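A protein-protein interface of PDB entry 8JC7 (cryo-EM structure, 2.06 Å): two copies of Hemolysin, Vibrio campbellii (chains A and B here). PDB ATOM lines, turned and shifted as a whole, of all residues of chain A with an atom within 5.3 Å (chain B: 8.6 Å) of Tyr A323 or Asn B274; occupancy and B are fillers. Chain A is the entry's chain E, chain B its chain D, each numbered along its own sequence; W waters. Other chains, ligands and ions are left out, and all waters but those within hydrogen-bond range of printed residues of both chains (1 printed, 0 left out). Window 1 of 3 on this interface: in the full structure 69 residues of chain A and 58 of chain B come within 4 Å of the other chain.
The side-chain carboxylate of Asp A322 sits close to the side-chain amide oxygen of Asn B274 (2.5 Å). The side-chain amide nitrogen (ND2) of Asn B274 sits at hydrogen-bond distance from the backbone carbonyl oxygen (O) of Tyr A323, 3.0 Å away. The backbone NH (N) of Val B275 is in hydrogen-bond range of the side-chain carboxylate (OD1) of Asp A322, 3.2 Å away.
Printed residues of chain B within 4 Å of Tyr A323: Asn B274. Of the printed residues of chain A, Asn B274 touches Gln A321, Asp A322, Tyr A323 and Leu A373. No residue of chain B comes within 4 Å of Ala A248. Of chain B, only Asn B274 (2.5 Å), Val B275 (3.2 Å) and Tyr B277 (3.9 Å) come within 4 Å of Asp A322. Ser A374 touches none of the printed residues of chain B. Printed residues of chain A within 4 Å of Tyr B277: Asp A322. Printed residues of chain A within 4 Å of Asn B272: Leu A373. Of the printed residues of chain A, Asp B271 touches Leu A373 (3.5 Å). Printed residues of chain A within 4 Å of Leu B273: Leu A373. Printed residues of chain B within 4 Å of Gln A321: Asn B274, Val B275 and Lys B276.
Water W1 bridges the side-chain amide oxygen (OE1) of Gln A321 and the backbone carbonyl oxygen (O) of Asn B274.
Positions printed for both chains: 324 and 325.
The side-chain hydroxyl (OH) of Tyr A323 is in hydrogen-bond range of the backbone carbonyl oxygen (O) of Ala A248 (2.5 Å). The side-chain hydroxyl of Tyr A251 sits at hydrogen-bond distance from the backbone carbonyl oxygen of Leu A373, 2.8 Å away. N of Gln A321 is in hydrogen-bond range of OE1 of Gln A342. The backbone carbonyl oxygen (O) of Asp A322 lies within hydrogen-bond range of the backbone NH (N) of Gln A342 (2.9 Å). The side-chain hydroxyl (OG) of Ser A371 is in hydrogen-bond range of the side-chain carboxylate (OD2) of Asp A322, 2.8 Å away. The side-chain hydroxyl of Tyr A323 sits at hydrogen-bond distance from the guanidinium group of Arg A341 (3.4 Å).
Asn B274 touches Gln A321. Val B275 touches Gln A321 (O to CA, 3.2 Å). Gln A321 touches Lys B276. Asp A322 touches Tyr B277. Asp B271 touches Leu A373. Leu A373 touches Asn B272. Leu A373 touches Leu B273 (CD2 to O, 3.8 Å). Asn B274 touches Leu A373 (CA to CD2, 3.8 Å).
Hydrophobic or aromatic side chains of chain A that line the printed part of chain B: Tyr A323 and Leu A373. Hydrophobic or aromatic side chains of chain B within 4 Å of the printed part of chain A: Tyr B277. Among the printed residues, 11 pairs touch across the chains. Among the printed residues, no Asp or Glu carboxylate lies within 4 Å of a Lys or Arg side-chain nitrogen of the other chain.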
ATOM      1  N   ALA A 248     -15.019  19.367  -0.622  1.00  0.00           N
ATOM      2  CA  ALA A 248     -16.002  18.311  -0.787  1.00  0.00           C
ATOM      3  C   ALA A 248     -15.370  17.194  -1.594  1.00  0.00           C
ATOM      4  O   ALA A 248     -15.081  17.367  -2.778  1.00  0.00           O
ATOM      5  CB  ALA A 248     -17.251  18.837  -1.476  1.00  0.00           C
ATOM      6  N   GLN A 249     -15.138  16.054  -0.952  1.00  0.00           N
ATOM      7  CA  GLN A 249     -14.677  14.893  -1.694  1.00  0.00           C
ATOM      8  C   GLN A 249     -15.729  14.444  -2.687  1.00  0.00           C
ATOM      9  O   GLN A 249     -15.408  14.070  -3.816  1.00  0.00           O
ATOM     10  CB  GLN A 249     -14.317  13.763  -0.741  1.00  0.00           C
ATOM     11  CG  GLN A 249     -13.554  12.646  -1.390  1.00  0.00           C
ATOM     12  CD  GLN A 249     -12.272  13.113  -2.023  1.00  0.00           C
ATOM     13  OE1 GLN A 249     -11.586  13.974  -1.494  1.00  0.00           O
ATOM     14  NE2 GLN A 249     -11.934  12.539  -3.158  1.00  0.00           N
ATOM     15  N   ASP A 250     -16.994  14.473  -2.287  1.00  0.00           N
ATOM     16  CA  ASP A 250     -18.074  14.189  -3.211  1.00  0.00           C
ATOM     17  C   ASP A 250     -19.363  14.779  -2.678  1.00  0.00           C
ATOM     18  O   ASP A 250     -19.485  15.088  -1.496  1.00  0.00           O
ATOM     19  CB  ASP A 250     -18.235  12.693  -3.442  1.00  0.00           C
ATOM     20  CG  ASP A 250     -18.555  11.947  -2.190  1.00  0.00           C
ATOM     21  OD1 ASP A 250     -19.716  11.998  -1.746  1.00  0.00           O
ATOM     22  OD2 ASP A 250     -17.647  11.292  -1.646  1.00  0.00           O
ATOM     23  N   TYR A 251     -20.317  14.941  -3.580  1.00  0.00           N
ATOM     24  CA  TYR A 251     -21.690  15.268  -3.243  1.00  0.00           C
ATOM     25  C   TYR A 251     -22.568  14.114  -3.680  1.00  0.00           C
ATOM     26  O   TYR A 251     -22.489  13.680  -4.827  1.00  0.00           O
ATOM     27  CB  TYR A 251     -22.142  16.544  -3.936  1.00  0.00           C
ATOM     28  CG  TYR A 251     -21.217  17.711  -3.810  1.00  0.00           C
ATOM     29  CD1 TYR A 251     -21.356  18.614  -2.784  1.00  0.00           C
ATOM     30  CD2 TYR A 251     -20.226  17.931  -4.739  1.00  0.00           C
ATOM     31  CE1 TYR A 251     -20.534  19.684  -2.678  1.00  0.00           C
ATOM     32  CE2 TYR A 251     -19.398  18.998  -4.638  1.00  0.00           C
ATOM     33  CZ  TYR A 251     -19.557  19.875  -3.609  1.00  0.00           C
ATOM     34  OH  TYR A 251     -18.727  20.952  -3.503  1.00  0.00           O
ATOM     35  N   GLN A 321     -12.857  15.198 -15.755  1.00  0.00           N
ATOM     36  CA  GLN A 321     -13.362  16.406 -15.130  1.00  0.00           C
ATOM     37  C   GLN A 321     -12.875  16.423 -13.699  1.00  0.00           C
ATOM     38  O   GLN A 321     -12.348  15.433 -13.202  1.00  0.00           O
ATOM     39  CB  GLN A 321     -14.884  16.469 -15.167  1.00  0.00           C
ATOM     40  CG  GLN A 321     -15.476  16.092 -16.477  1.00  0.00           C
ATOM     41  CD  GLN A 321     -16.894  15.633 -16.340  1.00  0.00           C
ATOM     42  OE1 GLN A 321     -17.823  16.419 -16.476  1.00  0.00           O
ATOM     43  NE2 GLN A 321     -17.075  14.356 -16.064  1.00  0.00           N
ATOM     44  N   ASP A 322     -13.027  17.550 -13.022  1.00  0.00           N
ATOM     45  CA  ASP A 322     -12.696  17.498 -11.611  1.00  0.00           C
ATOM     46  C   ASP A 322     -13.815  16.908 -10.777  1.00  0.00           C
ATOM     47  O   ASP A 322     -13.561  16.486  -9.652  1.00  0.00           O
ATOM     48  CB  ASP A 322     -12.312  18.870 -11.074  1.00  0.00           C
ATOM     49  CG  ASP A 322     -13.275  19.906 -11.448  1.00  0.00           C
ATOM     50  OD1 ASP A 322     -14.015  19.649 -12.399  1.00  0.00           O
ATOM     51  OD2 ASP A 322     -13.313  20.962 -10.792  1.00  0.00           O
ATOM     52  N   TYR A 323     -15.033  16.837 -11.302  1.00  0.00           N
ATOM     53  CA  TYR A 323     -16.106  16.108 -10.643  1.00  0.00           C
ATOM     54  C   TYR A 323     -16.806  15.254 -11.678  1.00  0.00           C
ATOM     55  O   TYR A 323     -17.299  15.774 -12.677  1.00  0.00           O
ATOM     56  CB  TYR A 323     -17.094  17.052  -9.967  1.00  0.00           C
ATOM     57  CG  TYR A 323     -16.641  17.477  -8.609  1.00  0.00           C
ATOM     58  CD1 TYR A 323     -15.897  18.622  -8.442  1.00  0.00           C
ATOM     59  CD2 TYR A 323     -16.933  16.725  -7.501  1.00  0.00           C
ATOM     60  CE1 TYR A 323     -15.470  19.004  -7.217  1.00  0.00           C
ATOM     61  CE2 TYR A 323     -16.511  17.102  -6.274  1.00  0.00           C
ATOM     62  CZ  TYR A 323     -15.781  18.242  -6.135  1.00  0.00           C
ATOM     63  OH  TYR A 323     -15.354  18.624  -4.900  1.00  0.00           O
ATOM     64  N   ARG A 324     -16.846  13.954 -11.443  1.00  0.00           N
ATOM     65  CA  ARG A 324     -17.497  13.016 -12.337  1.00  0.00           C
ATOM     66  C   ARG A 324     -18.773  12.502 -11.697  1.00  0.00           C
ATOM     67  O   ARG A 324     -18.774  12.114 -10.530  1.00  0.00           O
ATOM     68  CB  ARG A 324     -16.577  11.849 -12.662  1.00  0.00           C
ATOM     69  CG  ARG A 324     -17.229  10.797 -13.501  1.00  0.00           C
ATOM     70  CD  ARG A 324     -16.282   9.685 -13.816  1.00  0.00           C
ATOM     71  NE  ARG A 324     -15.864   8.976 -12.620  1.00  0.00           N
ATOM     72  CZ  ARG A 324     -14.975   7.996 -12.620  1.00  0.00           C
ATOM     73  NH1 ARG A 324     -14.416   7.614 -13.753  1.00  0.00           N
ATOM     74  NH2 ARG A 324     -14.647   7.399 -11.491  1.00  0.00           N
ATOM     75  N   VAL A 325     -19.854  12.501 -12.457  1.00  0.00           N
ATOM     76  CA  VAL A 325     -21.133  11.995 -11.981  1.00  0.00           C
ATOM     77  C   VAL A 325     -21.121  10.483 -12.061  1.00  0.00           C
ATOM     78  O   VAL A 325     -20.834   9.912 -13.114  1.00  0.00           O
ATOM     79  CB  VAL A 325     -22.296  12.562 -12.802  1.00  0.00           C
ATOM     80  CG1 VAL A 325     -23.570  12.466 -12.012  1.00  0.00           C
ATOM     81  CG2 VAL A 325     -22.013  13.970 -13.202  1.00  0.00           C
ATOM     82  N   TRP A 339     -21.444  13.099  -7.345  1.00  0.00           N
ATOM     83  CA  TRP A 339     -20.420  13.867  -8.030  1.00  0.00           C
ATOM     84  C   TRP A 339     -19.126  13.668  -7.263  1.00  0.00           C
ATOM     85  O   TRP A 339     -18.963  14.195  -6.168  1.00  0.00           O
ATOM     86  CB  TRP A 339     -20.795  15.336  -8.112  1.00  0.00           C
ATOM     87  CG  TRP A 339     -21.733  15.620  -9.196  1.00  0.00           C
ATOM     88  CD1 TRP A 339     -21.446  16.193 -10.381  1.00  0.00           C
ATOM     89  CD2 TRP A 339     -23.130  15.351  -9.205  1.00  0.00           C
ATOM     90  NE1 TRP A 339     -22.573  16.304 -11.135  1.00  0.00           N
ATOM     91  CE2 TRP A 339     -23.626  15.788 -10.433  1.00  0.00           C
ATOM     92  CE3 TRP A 339     -24.010  14.782  -8.291  1.00  0.00           C
ATOM     93  CZ2 TRP A 339     -24.958  15.675 -10.776  1.00  0.00           C
ATOM     94  CZ3 TRP A 339     -25.322  14.674  -8.630  1.00  0.00           C
ATOM     95  CH2 TRP A 339     -25.788  15.113  -9.860  1.00  0.00           C
ATOM     96  N   ASN A 340     -18.221  12.900  -7.832  1.00  0.00           N
ATOM     97  CA  ASN A 340     -17.006  12.481  -7.163  1.00  0.00           C
ATOM     98  C   ASN A 340     -15.821  13.215  -7.763  1.00  0.00           C
ATOM     99  O   ASN A 340     -15.741  13.380  -8.979  1.00  0.00           O
ATOM    100  CB  ASN A 340     -16.831  10.977  -7.315  1.00  0.00           C
ATOM    101  CG  ASN A 340     -16.154  10.356  -6.147  1.00  0.00           C
ATOM    102  OD1 ASN A 340     -16.062  10.948  -5.081  1.00  0.00           O
ATOM    103  ND2 ASN A 340     -15.661   9.147  -6.334  1.00  0.00           N
ATOM    104  N   ARG A 341     -14.910  13.672  -6.911  1.00  0.00           N
ATOM    105  CA  ARG A 341     -13.684  14.284  -7.401  1.00  0.00           C
ATOM    106  C   ARG A 341     -12.927  13.297  -8.269  1.00  0.00           C
ATOM    107  O   ARG A 341     -12.696  12.157  -7.868  1.00  0.00           O
ATOM    108  CB  ARG A 341     -12.803  14.724  -6.241  1.00  0.00           C
ATOM    109  CG  ARG A 341     -13.161  16.044  -5.665  1.00  0.00           C
ATOM    110  CD  ARG A 341     -12.171  16.467  -4.618  1.00  0.00           C
ATOM    111  NE  ARG A 341     -10.993  17.070  -5.214  1.00  0.00           N
ATOM    112  CZ  ARG A 341     -10.949  18.304  -5.687  1.00  0.00           C
ATOM    113  NH1 ARG A 341     -12.017  19.070  -5.634  1.00  0.00           N
ATOM    114  NH2 ARG A 341      -9.836  18.772  -6.214  1.00  0.00           N
ATOM    115  N   GLN A 342     -12.547  13.726  -9.466  1.00  0.00           N
ATOM    116  CA  GLN A 342     -11.846  12.834 -10.374  1.00  0.00           C
ATOM    117  C   GLN A 342     -10.430  13.300 -10.681  1.00  0.00           C
ATOM    118  O   GLN A 342      -9.482  12.567 -10.403  1.00  0.00           O
ATOM    119  CB  GLN A 342     -12.638  12.662 -11.669  1.00  0.00           C
ATOM    120  CG  GLN A 342     -11.942  11.782 -12.663  1.00  0.00           C
ATOM    121  CD  GLN A 342     -12.704  11.628 -13.944  1.00  0.00           C
ATOM    122  OE1 GLN A 342     -13.389  12.537 -14.383  1.00  0.00           O
ATOM    123  NE2 GLN A 342     -12.582  10.471 -14.559  1.00  0.00           N
ATOM    124  N   SER A 371     -10.945  23.926  -7.512  1.00  0.00           N
ATOM    125  CA  SER A 371     -11.935  24.786  -8.117  1.00  0.00           C
ATOM    126  C   SER A 371     -12.944  25.254  -7.080  1.00  0.00           C
ATOM    127  O   SER A 371     -13.141  24.606  -6.056  1.00  0.00           O
ATOM    128  CB  SER A 371     -12.655  24.047  -9.234  1.00  0.00           C
ATOM    129  OG  SER A 371     -13.237  22.859  -8.741  1.00  0.00           O
ATOM    130  N   LEU A 373     -15.952  24.963  -7.360  1.00  0.00           N
ATOM    131  CA  LEU A 373     -16.969  23.927  -7.335  1.00  0.00           C
ATOM    132  C   LEU A 373     -16.825  23.006  -6.139  1.00  0.00           C
ATOM    133  O   LEU A 373     -17.795  22.358  -5.747  1.00  0.00           O
ATOM    134  CB  LEU A 373     -16.894  23.115  -8.621  1.00  0.00           C
ATOM    135  CG  LEU A 373     -18.022  22.139  -8.898  1.00  0.00           C
ATOM    136  CD1 LEU A 373     -19.326  22.873  -8.935  1.00  0.00           C
ATOM    137  CD2 LEU A 373     -17.774  21.445 -10.194  1.00  0.00           C
ATOM    138  N   SER A 374     -15.646  22.934  -5.547  1.00  0.00           N
ATOM    139  CA  SER A 374     -15.407  21.992  -4.470  1.00  0.00           C
ATOM    140  C   SER A 374     -15.630  22.576  -3.086  1.00  0.00           C
ATOM    141  O   SER A 374     -15.662  21.822  -2.115  1.00  0.00           O
ATOM    142  CB  SER A 374     -13.993  21.440  -4.583  1.00  0.00           C
ATOM    143  OG  SER A 374     -13.070  22.483  -4.705  1.00  0.00           O
ATOM    144  N   ASP B 271     -24.033  27.515 -12.159  1.00  0.00           N
ATOM    145  CA  ASP B 271     -23.168  26.895 -11.172  1.00  0.00           C
ATOM    146  C   ASP B 271     -21.729  27.254 -11.489  1.00  0.00           C
ATOM    147  O   ASP B 271     -21.432  27.864 -12.515  1.00  0.00           O
ATOM    148  CB  ASP B 271     -23.352  25.377 -11.146  1.00  0.00           C
ATOM    149  CG  ASP B 271     -22.756  24.739  -9.906  1.00  0.00           C
ATOM    150  OD1 ASP B 271     -22.653  23.495  -9.858  1.00  0.00           O
ATOM    151  OD2 ASP B 271     -22.372  25.490  -8.986  1.00  0.00           O
ATOM    152  N   ASN B 272     -20.842  26.875 -10.581  1.00  0.00           N
ATOM    153  CA  ASN B 272     -19.420  26.957 -10.845  1.00  0.00           C
ATOM    154  C   ASN B 272     -19.033  25.966 -11.932  1.00  0.00           C
ATOM    155  O   ASN B 272     -19.690  24.948 -12.139  1.00  0.00           O
ATOM    156  CB  ASN B 272     -18.634  26.685  -9.572  1.00  0.00           C
ATOM    157  CG  ASN B 272     -18.699  27.827  -8.609  1.00  0.00           C
ATOM    158  OD1 ASN B 272     -18.314  28.936  -8.935  1.00  0.00           O
ATOM    159  ND2 ASN B 272     -19.190  27.570  -7.418  1.00  0.00           N
ATOM    160  N   LEU B 273     -17.958  26.284 -12.637  1.00  0.00           N
ATOM    161  CA  LEU B 273     -17.542  25.481 -13.774  1.00  0.00           C
ATOM    162  C   LEU B 273     -16.991  24.132 -13.336  1.00  0.00           C
ATOM    163  O   LEU B 273     -16.198  24.041 -12.399  1.00  0.00           O
ATOM    164  CB  LEU B 273     -16.485  26.227 -14.573  1.00  0.00           C
ATOM    165  CG  LEU B 273     -16.656  26.233 -16.083  1.00  0.00           C
ATOM    166  CD1 LEU B 273     -18.126  26.300 -16.436  1.00  0.00           C
ATOM    167  CD2 LEU B 273     -15.913  27.408 -16.666  1.00  0.00           C
ATOM    168  N   ASN B 274     -17.411  23.083 -14.032  1.00  0.00           N
ATOM    169  CA  ASN B 274     -16.845  21.745 -13.880  1.00  0.00           C
ATOM    170  C   ASN B 274     -15.779  21.601 -14.954  1.00  0.00           C
ATOM    171  O   ASN B 274     -16.064  21.270 -16.100  1.00  0.00           O
ATOM    172  CB  ASN B 274     -17.937  20.693 -14.006  1.00  0.00           C
ATOM    173  CG  ASN B 274     -17.530  19.358 -13.453  1.00  0.00           C
ATOM    174  OD1 ASN B 274     -16.385  19.140 -13.129  1.00  0.00           O
ATOM    175  ND2 ASN B 274     -18.476  18.450 -13.352  1.00  0.00           N
ATOM    176  N   VAL B 275     -14.527  21.866 -14.579  1.00  0.00           N
ATOM    177  CA  VAL B 275     -13.454  21.971 -15.559  1.00  0.00           C
ATOM    178  C   VAL B 275     -13.225  20.637 -16.249  1.00  0.00           C
ATOM    179  O   VAL B 275     -13.256  19.575 -15.624  1.00  0.00           O
ATOM    180  CB  VAL B 275     -12.167  22.467 -14.884  1.00  0.00           C
ATOM    181  CG1 VAL B 275     -11.046  22.552 -15.881  1.00  0.00           C
ATOM    182  CG2 VAL B 275     -12.396  23.810 -14.261  1.00  0.00           C
ATOM    183  N   LYS B 276     -12.996  20.693 -17.552  1.00  0.00           N
ATOM    184  CA  LYS B 276     -12.736  19.518 -18.363  1.00  0.00           C
ATOM    185  C   LYS B 276     -11.253  19.448 -18.694  1.00  0.00           C
ATOM    186  O   LYS B 276     -10.683  20.414 -19.202  1.00  0.00           O
ATOM    187  CB  LYS B 276     -13.565  19.569 -19.640  1.00  0.00           C
ATOM    188  CG  LYS B 276     -13.195  18.529 -20.660  1.00  0.00           C
ATOM    189  CD  LYS B 276     -13.908  17.226 -20.381  1.00  0.00           C
ATOM    190  CE  LYS B 276     -15.388  17.447 -20.149  1.00  0.00           C
ATOM    191  NZ  LYS B 276     -16.115  16.159 -20.044  1.00  0.00           N
ATOM    192  N   TYR B 277     -10.633  18.313 -18.406  1.00  0.00           N
ATOM    193  CA  TYR B 277      -9.213  18.112 -18.639  1.00  0.00           C
ATOM    194  C   TYR B 277      -9.008  17.084 -19.732  1.00  0.00           C
ATOM    195  O   TYR B 277      -9.749  16.109 -19.819  1.00  0.00           O
ATOM    196  CB  TYR B 277      -8.505  17.633 -17.381  1.00  0.00           C
ATOM    197  CG  TYR B 277      -8.634  18.562 -16.226  1.00  0.00           C
ATOM    198  CD1 TYR B 277      -9.683  18.447 -15.343  1.00  0.00           C
ATOM    199  CD2 TYR B 277      -7.710  19.558 -16.015  1.00  0.00           C
ATOM    200  CE1 TYR B 277      -9.804  19.290 -14.287  1.00  0.00           C
ATOM    201  CE2 TYR B 277      -7.826  20.407 -14.963  1.00  0.00           C
ATOM    202  CZ  TYR B 277      -8.876  20.270 -14.102  1.00  0.00           C
ATOM    203  OH  TYR B 277      -8.996  21.121 -13.040  1.00  0.00           O
ATOM    204  N   ARG B 324     -12.471  34.448 -14.122  1.00  0.00           N
ATOM    205  CA  ARG B 324     -13.308  33.286 -13.893  1.00  0.00           C
ATOM    206  C   ARG B 324     -14.451  33.656 -12.963  1.00  0.00           C
ATOM    207  O   ARG B 324     -14.236  34.296 -11.936  1.00  0.00           O
ATOM    208  CB  ARG B 324     -12.499  32.146 -13.291  1.00  0.00           C
ATOM    209  CG  ARG B 324     -13.331  30.957 -12.926  1.00  0.00           C
ATOM    210  CD  ARG B 324     -12.488  29.860 -12.363  1.00  0.00           C
ATOM    211  NE  ARG B 324     -11.858  30.252 -11.117  1.00  0.00           N
ATOM    212  CZ  ARG B 324     -11.006  29.487 -10.451  1.00  0.00           C
ATOM    213  NH1 ARG B 324     -10.690  28.294 -10.919  1.00  0.00           N
ATOM    214  NH2 ARG B 324     -10.475  29.914  -9.322  1.00  0.00           N
ATOM    215  N   VAL B 325     -15.658  33.257 -13.326  1.00  0.00           N
ATOM    216  CA  VAL B 325     -16.833  33.506 -12.505  1.00  0.00           C
ATOM    217  C   VAL B 325     -16.878  32.481 -11.391  1.00  0.00           C
ATOM    218  O   VAL B 325     -16.822  31.277 -11.645  1.00  0.00           O
ATOM    219  CB  VAL B 325     -18.116  33.442 -13.338  1.00  0.00           C
ATOM    220  CG1 VAL B 325     -19.217  34.185 -12.635  1.00  0.00           C
ATOM    221  CG2 VAL B 325     -17.877  33.995 -14.704  1.00  0.00           C
HETATM  222  O   HOH W   1     -17.161  18.840 -17.139  1.00  0.00           O
